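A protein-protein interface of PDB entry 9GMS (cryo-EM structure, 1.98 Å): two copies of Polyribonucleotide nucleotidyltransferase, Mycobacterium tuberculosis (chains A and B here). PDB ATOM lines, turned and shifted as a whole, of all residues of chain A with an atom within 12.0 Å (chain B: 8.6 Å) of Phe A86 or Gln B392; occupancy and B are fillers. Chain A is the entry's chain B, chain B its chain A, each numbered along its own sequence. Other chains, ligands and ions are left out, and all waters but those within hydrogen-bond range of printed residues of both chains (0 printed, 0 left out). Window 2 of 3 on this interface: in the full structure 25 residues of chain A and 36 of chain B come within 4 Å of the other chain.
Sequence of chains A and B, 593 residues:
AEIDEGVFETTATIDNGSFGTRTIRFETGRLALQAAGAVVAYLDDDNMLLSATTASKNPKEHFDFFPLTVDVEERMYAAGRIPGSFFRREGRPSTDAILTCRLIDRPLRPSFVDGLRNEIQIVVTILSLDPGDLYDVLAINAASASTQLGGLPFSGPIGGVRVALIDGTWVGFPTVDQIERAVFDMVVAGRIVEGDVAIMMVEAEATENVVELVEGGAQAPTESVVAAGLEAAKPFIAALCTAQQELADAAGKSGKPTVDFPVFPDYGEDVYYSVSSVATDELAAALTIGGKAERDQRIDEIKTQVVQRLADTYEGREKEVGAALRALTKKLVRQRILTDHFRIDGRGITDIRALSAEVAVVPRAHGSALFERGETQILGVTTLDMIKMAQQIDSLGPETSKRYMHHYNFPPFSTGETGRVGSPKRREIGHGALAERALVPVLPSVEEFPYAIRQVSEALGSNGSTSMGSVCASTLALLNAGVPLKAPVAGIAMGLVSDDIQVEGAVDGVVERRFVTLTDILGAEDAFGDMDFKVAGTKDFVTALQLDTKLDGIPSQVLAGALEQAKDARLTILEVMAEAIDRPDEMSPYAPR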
ATOM      1  N   MET A  76      12.263  27.322  -0.718  1.00  0.00           N
ATOM      2  CA  MET A  76      13.432  28.013  -0.191  1.00  0.00           C
ATOM      3  C   MET A  76      14.715  27.623  -0.915  1.00  0.00           C
ATOM      4  O   MET A  76      15.640  28.438  -0.982  1.00  0.00           O
ATOM      5  CB  MET A  76      13.573  27.734   1.304  1.00  0.00           C
ATOM      6  CG  MET A  76      14.175  28.878   2.086  1.00  0.00           C
ATOM      7  SD  MET A  76      13.165  30.373   2.056  1.00  0.00           S
ATOM      8  CE  MET A  76      14.325  31.497   1.306  1.00  0.00           C
ATOM      9  N   ILE A  82      18.424  27.012   3.769  1.00  0.00           N
ATOM     10  CA  ILE A  82      17.479  26.177   4.512  1.00  0.00           C
ATOM     11  C   ILE A  82      16.498  27.063   5.275  1.00  0.00           C
ATOM     12  O   ILE A  82      16.902  28.103   5.810  1.00  0.00           O
ATOM     13  CB  ILE A  82      18.234  25.224   5.455  1.00  0.00           C
ATOM     14  CG1 ILE A  82      19.112  24.274   4.638  1.00  0.00           C
ATOM     15  CG2 ILE A  82      17.274  24.428   6.335  1.00  0.00           C
ATOM     16  CD1 ILE A  82      19.916  23.308   5.464  1.00  0.00           C
ATOM     17  N   PRO A  83      15.216  26.695   5.376  1.00  0.00           N
ATOM     18  CA  PRO A  83      14.261  27.549   6.096  1.00  0.00           C
ATOM     19  C   PRO A  83      14.635  27.723   7.561  1.00  0.00           C
ATOM     20  O   PRO A  83      15.105  26.796   8.221  1.00  0.00           O
ATOM     21  CB  PRO A  83      12.932  26.799   5.950  1.00  0.00           C
ATOM     22  CG  PRO A  83      13.112  25.914   4.785  1.00  0.00           C
ATOM     23  CD  PRO A  83      14.551  25.528   4.775  1.00  0.00           C
ATOM     24  N   GLY A  84      14.390  28.926   8.072  1.00  0.00           N
ATOM     25  CA  GLY A  84      14.755  29.298   9.421  1.00  0.00           C
ATOM     26  C   GLY A  84      13.758  28.954  10.503  1.00  0.00           C
ATOM     27  O   GLY A  84      14.039  29.193  11.678  1.00  0.00           O
ATOM     28  N   SER A  85      12.607  28.387  10.156  1.00  0.00           N
ATOM     29  CA  SER A  85      11.605  28.053  11.155  1.00  0.00           C
ATOM     30  C   SER A  85      12.063  26.865  12.002  1.00  0.00           C
ATOM     31  O   SER A  85      13.024  26.165  11.681  1.00  0.00           O
ATOM     32  CB  SER A  85      10.268  27.745  10.487  1.00  0.00           C
ATOM     33  OG  SER A  85      10.413  26.735   9.509  1.00  0.00           O
ATOM     34  N   PHE A  86      11.339  26.640  13.100  1.00  0.00           N
ATOM     35  CA  PHE A  86      11.754  25.637  14.076  1.00  0.00           C
ATOM     36  C   PHE A  86      11.720  24.231  13.486  1.00  0.00           C
ATOM     37  O   PHE A  86      12.529  23.376  13.862  1.00  0.00           O
ATOM     38  CB  PHE A  86      10.868  25.726  15.319  1.00  0.00           C
ATOM     39  CG  PHE A  86      11.286  24.806  16.429  1.00  0.00           C
ATOM     40  CD1 PHE A  86      12.426  25.059  17.161  1.00  0.00           C
ATOM     41  CD2 PHE A  86      10.528  23.695  16.747  1.00  0.00           C
ATOM     42  CE1 PHE A  86      12.811  24.217  18.179  1.00  0.00           C
ATOM     43  CE2 PHE A  86      10.908  22.853  17.767  1.00  0.00           C
ATOM     44  CZ  PHE A  86      12.049  23.113  18.483  1.00  0.00           C
ATOM     45  N   PHE A  87      10.792  23.967  12.572  1.00  0.00           N
ATOM     46  CA  PHE A  87      10.696  22.667  11.924  1.00  0.00           C
ATOM     47  C   PHE A  87      11.407  22.613  10.577  1.00  0.00           C
ATOM     48  O   PHE A  87      11.343  21.581   9.905  1.00  0.00           O
ATOM     49  CB  PHE A  87       9.227  22.276  11.758  1.00  0.00           C
ATOM     50  CG  PHE A  87       8.519  22.073  13.063  1.00  0.00           C
ATOM     51  CD1 PHE A  87       8.682  20.902  13.778  1.00  0.00           C
ATOM     52  CD2 PHE A  87       7.710  23.062  13.590  1.00  0.00           C
ATOM     53  CE1 PHE A  87       8.044  20.716  14.985  1.00  0.00           C
ATOM     54  CE2 PHE A  87       7.069  22.882  14.795  1.00  0.00           C
ATOM     55  CZ  PHE A  87       7.236  21.707  15.494  1.00  0.00           C
ATOM     56  N   ARG A  88      12.084  23.688  10.173  1.00  0.00           N
ATOM     57  CA  ARG A  88      12.932  23.702   8.979  1.00  0.00           C
ATOM     58  C   ARG A  88      12.152  23.379   7.703  1.00  0.00           C
ATOM     59  O   ARG A  88      12.689  22.764   6.783  1.00  0.00           O
ATOM     60  CB  ARG A  88      14.108  22.731   9.129  1.00  0.00           C
ATOM     61  CG  ARG A  88      15.029  22.998  10.313  1.00  0.00           C
ATOM     62  CD  ARG A  88      15.845  24.260  10.115  1.00  0.00           C
ATOM     63  NE  ARG A  88      16.893  24.417  11.118  1.00  0.00           N
ATOM     64  CZ  ARG A  88      16.826  25.216  12.174  1.00  0.00           C
ATOM     65  NH1 ARG A  88      15.762  25.963  12.413  1.00  0.00           N
ATOM     66  NH2 ARG A  88      17.856  25.270  13.010  1.00  0.00           N
ATOM     67  N   ARG A  89      10.892  23.802   7.616  1.00  0.00           N
ATOM     68  CA  ARG A  89      10.073  23.502   6.451  1.00  0.00           C
ATOM     69  C   ARG A  89       9.123  24.664   6.187  1.00  0.00           C
ATOM     70  O   ARG A  89       8.707  25.362   7.115  1.00  0.00           O
ATOM     71  CB  ARG A  89       9.297  22.194   6.657  1.00  0.00           C
ATOM     72  CG  ARG A  89       8.611  21.662   5.417  1.00  0.00           C
ATOM     73  CD  ARG A  89       8.088  20.251   5.624  1.00  0.00           C
ATOM     74  NE  ARG A  89       7.516  19.704   4.401  1.00  0.00           N
ATOM     75  CZ  ARG A  89       7.234  18.424   4.202  1.00  0.00           C
ATOM     76  NH1 ARG A  89       7.447  17.513   5.134  1.00  0.00           N
ATOM     77  NH2 ARG A  89       6.728  18.049   3.033  1.00  0.00           N
ATOM     78  N   GLU A  90       8.780  24.865   4.915  1.00  0.00           N
ATOM     79  CA  GLU A  90       7.911  25.977   4.541  1.00  0.00           C
ATOM     80  C   GLU A  90       6.512  25.791   5.118  1.00  0.00           C
ATOM     81  O   GLU A  90       5.934  24.704   5.050  1.00  0.00           O
ATOM     82  CB  GLU A  90       7.816  26.108   3.018  1.00  0.00           C
ATOM     83  CG  GLU A  90       9.120  26.442   2.305  1.00  0.00           C
ATOM     84  CD  GLU A  90       9.914  25.212   1.902  1.00  0.00           C
ATOM     85  OE1 GLU A  90       9.572  24.101   2.346  1.00  0.00           O
ATOM     86  OE2 GLU A  90      10.882  25.360   1.131  1.00  0.00           O
ATOM     87  N   GLY A  91       5.955  26.873   5.658  1.00  0.00           N
ATOM     88  CA  GLY A  91       4.664  26.821   6.321  1.00  0.00           C
ATOM     89  C   GLY A  91       3.543  27.498   5.557  1.00  0.00           C
ATOM     90  O   GLY A  91       3.276  27.161   4.401  1.00  0.00           O
ATOM     91  N   ARG A  92       2.864  28.446   6.204  1.00  0.00           N
ATOM     92  CA  ARG A  92       1.811  29.202   5.551  1.00  0.00           C
ATOM     93  C   ARG A  92       2.401  30.159   4.513  1.00  0.00           C
ATOM     94  O   ARG A  92       3.544  30.597   4.642  1.00  0.00           O
ATOM     95  CB  ARG A  92       1.009  29.999   6.578  1.00  0.00           C
ATOM     96  CG  ARG A  92       0.241  29.173   7.608  1.00  0.00           C
ATOM     97  CD  ARG A  92      -0.746  28.197   6.976  1.00  0.00           C
ATOM     98  NE  ARG A  92      -0.112  26.992   6.450  1.00  0.00           N
ATOM     99  CZ  ARG A  92      -0.686  26.167   5.587  1.00  0.00           C
ATOM    100  NH1 ARG A  92      -1.898  26.397   5.111  1.00  0.00           N
ATOM    101  NH2 ARG A  92      -0.023  25.087   5.183  1.00  0.00           N
ATOM    102  N   ASP A 394      11.971  36.735   6.405  1.00  0.00           N
ATOM    103  CA  ASP A 394      12.775  35.627   5.894  1.00  0.00           C
ATOM    104  C   ASP A 394      11.999  34.996   4.741  1.00  0.00           C
ATOM    105  O   ASP A 394      11.109  34.174   4.969  1.00  0.00           O
ATOM    106  CB  ASP A 394      13.066  34.612   6.995  1.00  0.00           C
ATOM    107  CG  ASP A 394      13.930  33.462   6.520  1.00  0.00           C
ATOM    108  OD1 ASP A 394      14.508  33.563   5.420  1.00  0.00           O
ATOM    109  OD2 ASP A 394      14.025  32.452   7.243  1.00  0.00           O
ATOM    110  N   GLY B  84       9.048  22.816  26.008  1.00  0.00           N
ATOM    111  CA  GLY B  84       9.842  23.976  25.674  1.00  0.00           C
ATOM    112  C   GLY B  84       9.160  25.034  24.840  1.00  0.00           C
ATOM    113  O   GLY B  84       9.762  26.080  24.592  1.00  0.00           O
ATOM    114  N   SER B  85       7.925  24.811  24.400  1.00  0.00           N
ATOM    115  CA  SER B  85       7.255  25.762  23.527  1.00  0.00           C
ATOM    116  C   SER B  85       6.838  27.011  24.304  1.00  0.00           C
ATOM    117  O   SER B  85       6.876  27.059  25.535  1.00  0.00           O
ATOM    118  CB  SER B  85       6.042  25.113  22.865  1.00  0.00           C
ATOM    119  OG  SER B  85       5.127  24.629  23.829  1.00  0.00           O
ATOM    120  N   ARG B  92       0.719  20.330  18.219  1.00  0.00           N
ATOM    121  CA  ARG B  92       0.421  19.381  17.163  1.00  0.00           C
ATOM    122  C   ARG B  92       1.344  18.165  17.270  1.00  0.00           C
ATOM    123  O   ARG B  92       2.476  18.280  17.743  1.00  0.00           O
ATOM    124  CB  ARG B  92       0.571  20.042  15.793  1.00  0.00           C
ATOM    125  CG  ARG B  92       2.012  20.343  15.363  1.00  0.00           C
ATOM    126  CD  ARG B  92       2.073  20.825  13.911  1.00  0.00           C
ATOM    127  NE  ARG B  92       3.371  20.578  13.285  1.00  0.00           N
ATOM    128  CZ  ARG B  92       4.261  21.511  12.965  1.00  0.00           C
ATOM    129  NH1 ARG B  92       4.047  22.794  13.211  1.00  0.00           N
ATOM    130  NH2 ARG B  92       5.395  21.147  12.373  1.00  0.00           N
ATOM    131  N   MET B 386      25.394  25.740   6.807  1.00  0.00           N
ATOM    132  CA  MET B 386      26.240  25.595   7.986  1.00  0.00           C
ATOM    133  C   MET B 386      25.633  24.585   8.953  1.00  0.00           C
ATOM    134  O   MET B 386      24.415  24.419   9.027  1.00  0.00           O
ATOM    135  CB  MET B 386      26.409  26.939   8.696  1.00  0.00           C
ATOM    136  CG  MET B 386      27.037  28.049   7.867  1.00  0.00           C
ATOM    137  SD  MET B 386      28.838  28.002   7.823  1.00  0.00           S
ATOM    138  CE  MET B 386      29.149  26.917   6.435  1.00  0.00           C
ATOM    139  N   ILE B 387      26.500  23.923   9.721  1.00  0.00           N
ATOM    140  CA  ILE B 387      26.043  22.862  10.611  1.00  0.00           C
ATOM    141  C   ILE B 387      25.071  23.376  11.666  1.00  0.00           C
ATOM    142  O   ILE B 387      24.338  22.579  12.258  1.00  0.00           O
ATOM    143  CB  ILE B 387      27.249  22.168  11.273  1.00  0.00           C
ATOM    144  CG1 ILE B 387      26.844  20.824  11.878  1.00  0.00           C
ATOM    145  CG2 ILE B 387      27.840  23.040  12.362  1.00  0.00           C
ATOM    146  CD1 ILE B 387      26.467  19.777  10.861  1.00  0.00           C
ATOM    147  N   LYS B 388      25.033  24.685  11.926  1.00  0.00           N
ATOM    148  CA  LYS B 388      24.087  25.211  12.905  1.00  0.00           C
ATOM    149  C   LYS B 388      22.647  25.211  12.406  1.00  0.00           C
ATOM    150  O   LYS B 388      21.740  25.442  13.210  1.00  0.00           O
ATOM    151  CB  LYS B 388      24.475  26.630  13.325  1.00  0.00           C
ATOM    152  CG  LYS B 388      24.238  27.689  12.264  1.00  0.00           C
ATOM    153  CD  LYS B 388      24.774  29.043  12.692  1.00  0.00           C
ATOM    154  CE  LYS B 388      24.561  30.078  11.607  1.00  0.00           C
ATOM    155  NZ  LYS B 388      23.116  30.349  11.379  1.00  0.00           N
ATOM    156  N   MET B 389      22.408  24.973  11.119  1.00  0.00           N
ATOM    157  CA  MET B 389      21.049  24.897  10.602  1.00  0.00           C
ATOM    158  C   MET B 389      20.458  23.496  10.692  1.00  0.00           C
ATOM    159  O   MET B 389      19.381  23.262  10.138  1.00  0.00           O
ATOM    160  CB  MET B 389      20.988  25.383   9.148  1.00  0.00           C
ATOM    161  CG  MET B 389      21.312  26.858   8.960  1.00  0.00           C
ATOM    162  SD  MET B 389      20.363  27.973  10.015  1.00  0.00           S
ATOM    163  CE  MET B 389      18.678  27.576   9.571  1.00  0.00           C
ATOM    164  N   ALA B 390      21.130  22.562  11.358  1.00  0.00           N
ATOM    165  CA  ALA B 390      20.525  21.262  11.609  1.00  0.00           C
ATOM    166  C   ALA B 390      19.290  21.428  12.481  1.00  0.00           C
ATOM    167  O   ALA B 390      19.226  22.316  13.331  1.00  0.00           O
ATOM    168  CB  ALA B 390      21.520  20.323  12.287  1.00  0.00           C
ATOM    169  N   GLN B 391      18.298  20.579  12.252  1.00  0.00           N
ATOM    170  CA  GLN B 391      17.057  20.670  13.006  1.00  0.00           C
ATOM    171  C   GLN B 391      17.290  20.270  14.459  1.00  0.00           C
ATOM    172  O   GLN B 391      17.928  19.252  14.739  1.00  0.00           O
ATOM    173  CB  GLN B 391      15.990  19.785  12.370  1.00  0.00           C
ATOM    174  CG  GLN B 391      14.616  19.942  12.980  1.00  0.00           C
ATOM    175  CD  GLN B 391      13.590  19.042  12.334  1.00  0.00           C
ATOM    176  OE1 GLN B 391      13.892  18.313  11.396  1.00  0.00           O
ATOM    177  NE2 GLN B 391      12.367  19.086  12.836  1.00  0.00           N
ATOM    178  N   GLN B 392      16.780  21.078  15.382  1.00  0.00           N
ATOM    179  CA  GLN B 392      16.823  20.776  16.807  1.00  0.00           C
ATOM    180  C   GLN B 392      15.509  20.126  17.205  1.00  0.00           C
ATOM    181  O   GLN B 392      14.437  20.659  16.908  1.00  0.00           O
ATOM    182  CB  GLN B 392      17.053  22.043  17.634  1.00  0.00           C
ATOM    183  CG  GLN B 392      18.224  22.888  17.171  1.00  0.00           C
ATOM    184  CD  GLN B 392      19.525  22.115  17.135  1.00  0.00           C
ATOM    185  OE1 GLN B 392      19.796  21.294  18.009  1.00  0.00           O
ATOM    186  NE2 GLN B 392      20.334  22.365  16.115  1.00  0.00           N
ATOM    187  N   ILE B 393      15.590  18.978  17.867  1.00  0.00           N
ATOM    188  CA  ILE B 393      14.419  18.168  18.185  1.00  0.00           C
ATOM    189  C   ILE B 393      14.219  18.154  19.692  1.00  0.00           C
ATOM    190  O   ILE B 393      15.171  17.943  20.452  1.00  0.00           O
ATOM    191  CB  ILE B 393      14.555  16.743  17.627  1.00  0.00           C
ATOM    192  CG1 ILE B 393      14.550  16.795  16.100  1.00  0.00           C
ATOM    193  CG2 ILE B 393      13.415  15.880  18.128  1.00  0.00           C
ATOM    194  CD1 ILE B 393      15.100  15.573  15.450  1.00  0.00           C
ATOM    195  N   ASP B 394      12.979  18.387  20.115  1.00  0.00           N
ATOM    196  CA  ASP B 394      12.623  18.455  21.526  1.00  0.00           C
ATOM    197  C   ASP B 394      11.455  17.521  21.821  1.00  0.00           C
ATOM    198  O   ASP B 394      10.477  17.920  22.456  1.00  0.00           O
ATOM    199  CB  ASP B 394      12.287  19.898  21.908  1.00  0.00           C
ATOM    200  CG  ASP B 394      11.942  20.053  23.375  1.00  0.00           C
ATOM    201  OD1 ASP B 394      12.747  19.631  24.229  1.00  0.00           O
ATOM    202  OD2 ASP B 394      10.866  20.604  23.676  1.00  0.00           O
ATOM    203  N   SER B 395      11.538  16.283  21.348  1.00  0.00           N
ATOM    204  CA  SER B 395      10.460  15.319  21.471  1.00  0.00           C
ATOM    205  C   SER B 395      10.646  14.452  22.714  1.00  0.00           C
ATOM    206  O   SER B 395      11.527  14.670  23.545  1.00  0.00           O
ATOM    207  CB  SER B 395      10.389  14.437  20.227  1.00  0.00           C
ATOM    208  OG  SER B 395      11.551  13.635  20.124  1.00  0.00           O
ATOM    209  N   GLU B 399      16.100  10.959  20.287  1.00  0.00           N
ATOM    210  CA  GLU B 399      16.737  11.812  19.291  1.00  0.00           C
ATOM    211  C   GLU B 399      16.722  13.272  19.735  1.00  0.00           C
ATOM    212  O   GLU B 399      15.750  13.743  20.329  1.00  0.00           O
ATOM    213  CB  GLU B 399      16.020  11.659  17.951  1.00  0.00           C
ATOM    214  CG  GLU B 399      16.656  12.409  16.802  1.00  0.00           C
ATOM    215  CD  GLU B 399      15.898  12.231  15.499  1.00  0.00           C
ATOM    216  OE1 GLU B 399      14.661  12.068  15.546  1.00  0.00           O
ATOM    217  OE2 GLU B 399      16.540  12.246  14.429  1.00  0.00           O
ATOM    218  N   THR B 400      17.807  13.994  19.440  1.00  0.00           N
ATOM    219  CA  THR B 400      17.919  15.402  19.817  1.00  0.00           C
ATOM    220  C   THR B 400      18.260  16.347  18.673  1.00  0.00           C
ATOM    221  O   THR B 400      18.009  17.549  18.811  1.00  0.00           O
ATOM    222  CB  THR B 400      18.972  15.589  20.922  1.00  0.00           C
ATOM    223  OG1 THR B 400      20.197  14.956  20.539  1.00  0.00           O
ATOM    224  CG2 THR B 400      18.481  15.005  22.235  1.00  0.00           C
ATOM    225  N   SER B 401      18.829  15.870  17.569  1.00  0.00           N
ATOM    226  CA  SER B 401      19.091  16.728  16.422  1.00  0.00           C
ATOM    227  C   SER B 401      19.128  15.871  15.167  1.00  0.00           C
ATOM    228  O   SER B 401      19.343  14.659  15.227  1.00  0.00           O
ATOM    229  CB  SER B 401      20.399  17.510  16.584  1.00  0.00           C
ATOM    230  OG  SER B 401      21.517  16.646  16.566  1.00  0.00           O
ATOM    231  N   LYS B 402      18.924  16.517  14.021  1.00  0.00           N
ATOM    232  CA  LYS B 402      18.843  15.830  12.736  1.00  0.00           C
ATOM    233  C   LYS B 402      19.728  16.555  11.731  1.00  0.00           C
ATOM    234  O   LYS B 402      19.416  17.672  11.314  1.00  0.00           O
ATOM    235  CB  LYS B 402      17.401  15.759  12.242  1.00  0.00           C
ATOM    236  CG  LYS B 402      17.206  14.799  11.091  1.00  0.00           C
ATOM    237  CD  LYS B 402      15.857  14.977  10.422  1.00  0.00           C
ATOM    238  CE  LYS B 402      14.735  14.385  11.241  1.00  0.00           C
ATOM    239  NZ  LYS B 402      14.792  12.904  11.253  1.00  0.00           N
ATOM    240  N   ARG B 403      20.827  15.912  11.342  1.00  0.00           N
ATOM    241  CA  ARG B 403      21.768  16.519  10.408  1.00  0.00           C
ATOM    242  C   ARG B 403      21.261  16.454   8.967  1.00  0.00           C
ATOM    243  O   ARG B 403      21.497  17.376   8.182  1.00  0.00           O
ATOM    244  CB  ARG B 403      23.125  15.831  10.544  1.00  0.00           C
ATOM    245  CG  ARG B 403      24.195  16.319   9.600  1.00  0.00           C
ATOM    246  CD  ARG B 403      25.464  15.518   9.806  1.00  0.00           C
ATOM    247  NE  ARG B 403      26.555  15.948   8.938  1.00  0.00           N
ATOM    248  CZ  ARG B 403      26.888  15.367   7.792  1.00  0.00           C
ATOM    249  NH1 ARG B 403      26.213  14.336   7.315  1.00  0.00           N
ATOM    250  NH2 ARG B 403      27.931  15.830   7.112  1.00  0.00           N
ATOM    251  N   MET B 405      17.943  16.020   6.476  1.00  0.00           N
ATOM    252  CA  MET B 405      16.494  16.171   6.431  1.00  0.00           C
ATOM    253  C   MET B 405      15.994  15.848   5.030  1.00  0.00           C
ATOM    254  O   MET B 405      16.602  16.266   4.045  1.00  0.00           O
ATOM    255  CB  MET B 405      16.091  17.601   6.822  1.00  0.00           C
ATOM    256  CG  MET B 405      16.411  17.981   8.264  1.00  0.00           C
ATOM    257  SD  MET B 405      16.770  19.735   8.491  1.00  0.00           S
ATOM    258  CE  MET B 405      18.477  19.813   7.964  1.00  0.00           C
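Of the 13 printed residues of chain A, 4 touch a printed residue of chain B. Printed residues of chain A that touch a printed residue of chain B: Pro A83, Phe A86, Phe A87 and Arg A88.
The side-chain amide nitrogen (NE2) of Gln B392 lies within hydrogen-bond range of the backbone carbonyl oxygen (O) of Ala B390 (3.0 Å). O of Gln B391 is in hydrogen-bond range of N of Lys B402 (3.0 Å). The backbone carbonyl oxygen of Ser A85 sits at hydrogen-bond distance from the guanidinium group of Arg A88, 2.8 Å away.
4 positions are printed for both chains.
Among the printed residues, merely in contact across the chains: Phe A87 with Arg B92 (3.2 Å), Phe A86 with Gln B392 (3.8 Å), Arg A88 with Lys B388 (3.9 Å), Pro A83 with Met B389 (3.9 Å), Arg A88 with Gln B391 (3.9 Å) and Phe A87 with Gln B391 (3.98 Å).
The guanidinium group (NE) of Arg A88 lies within hydrogen-bond range of the backbone carbonyl oxygen (O) of Met B389, at 2.9 Å. The guanidinium group (NH2) of Arg A88 lies within hydrogen-bond range of the backbone carbonyl oxygen (O) of Ala B390, 3.3 Å away.
Of chain B, only Gln B392 comes within 4 Å of Phe A86. Of the printed residues of chain A, Gln B392 touches Phe A86. Ser A85 touches none of the printed residues of chain B. Ala B390 touches just one residue of chain A: Arg A88. No residue of chain A comes within 4 Å of Ile B393. No residue of chain A comes within 4 Å of Asp B394. No residue of chain A comes within 4 Å of Thr B400. Of the printed residues of chain B, Phe A87 touches Arg B92 and Gln B391. Printed residues of chain A within 4 Å of Gln B391: Phe A87 and Arg A88. Of the printed residues of chain B, Arg A88 touches Lys B388, Met B389, Ala B390 and Gln B391. Printed residues of chain B within 4 Å of Pro A83: Met B389. The nearest residue of chain B that does not touch Phe A86 is Gln B391 (4.1 Å). The nearest residue of chain A that does not touch Gln B392 is Arg A88 (4.8 Å). The nearest printed residue of chain A that does not touch Gln B391 is Phe A86 (4.1 Å).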
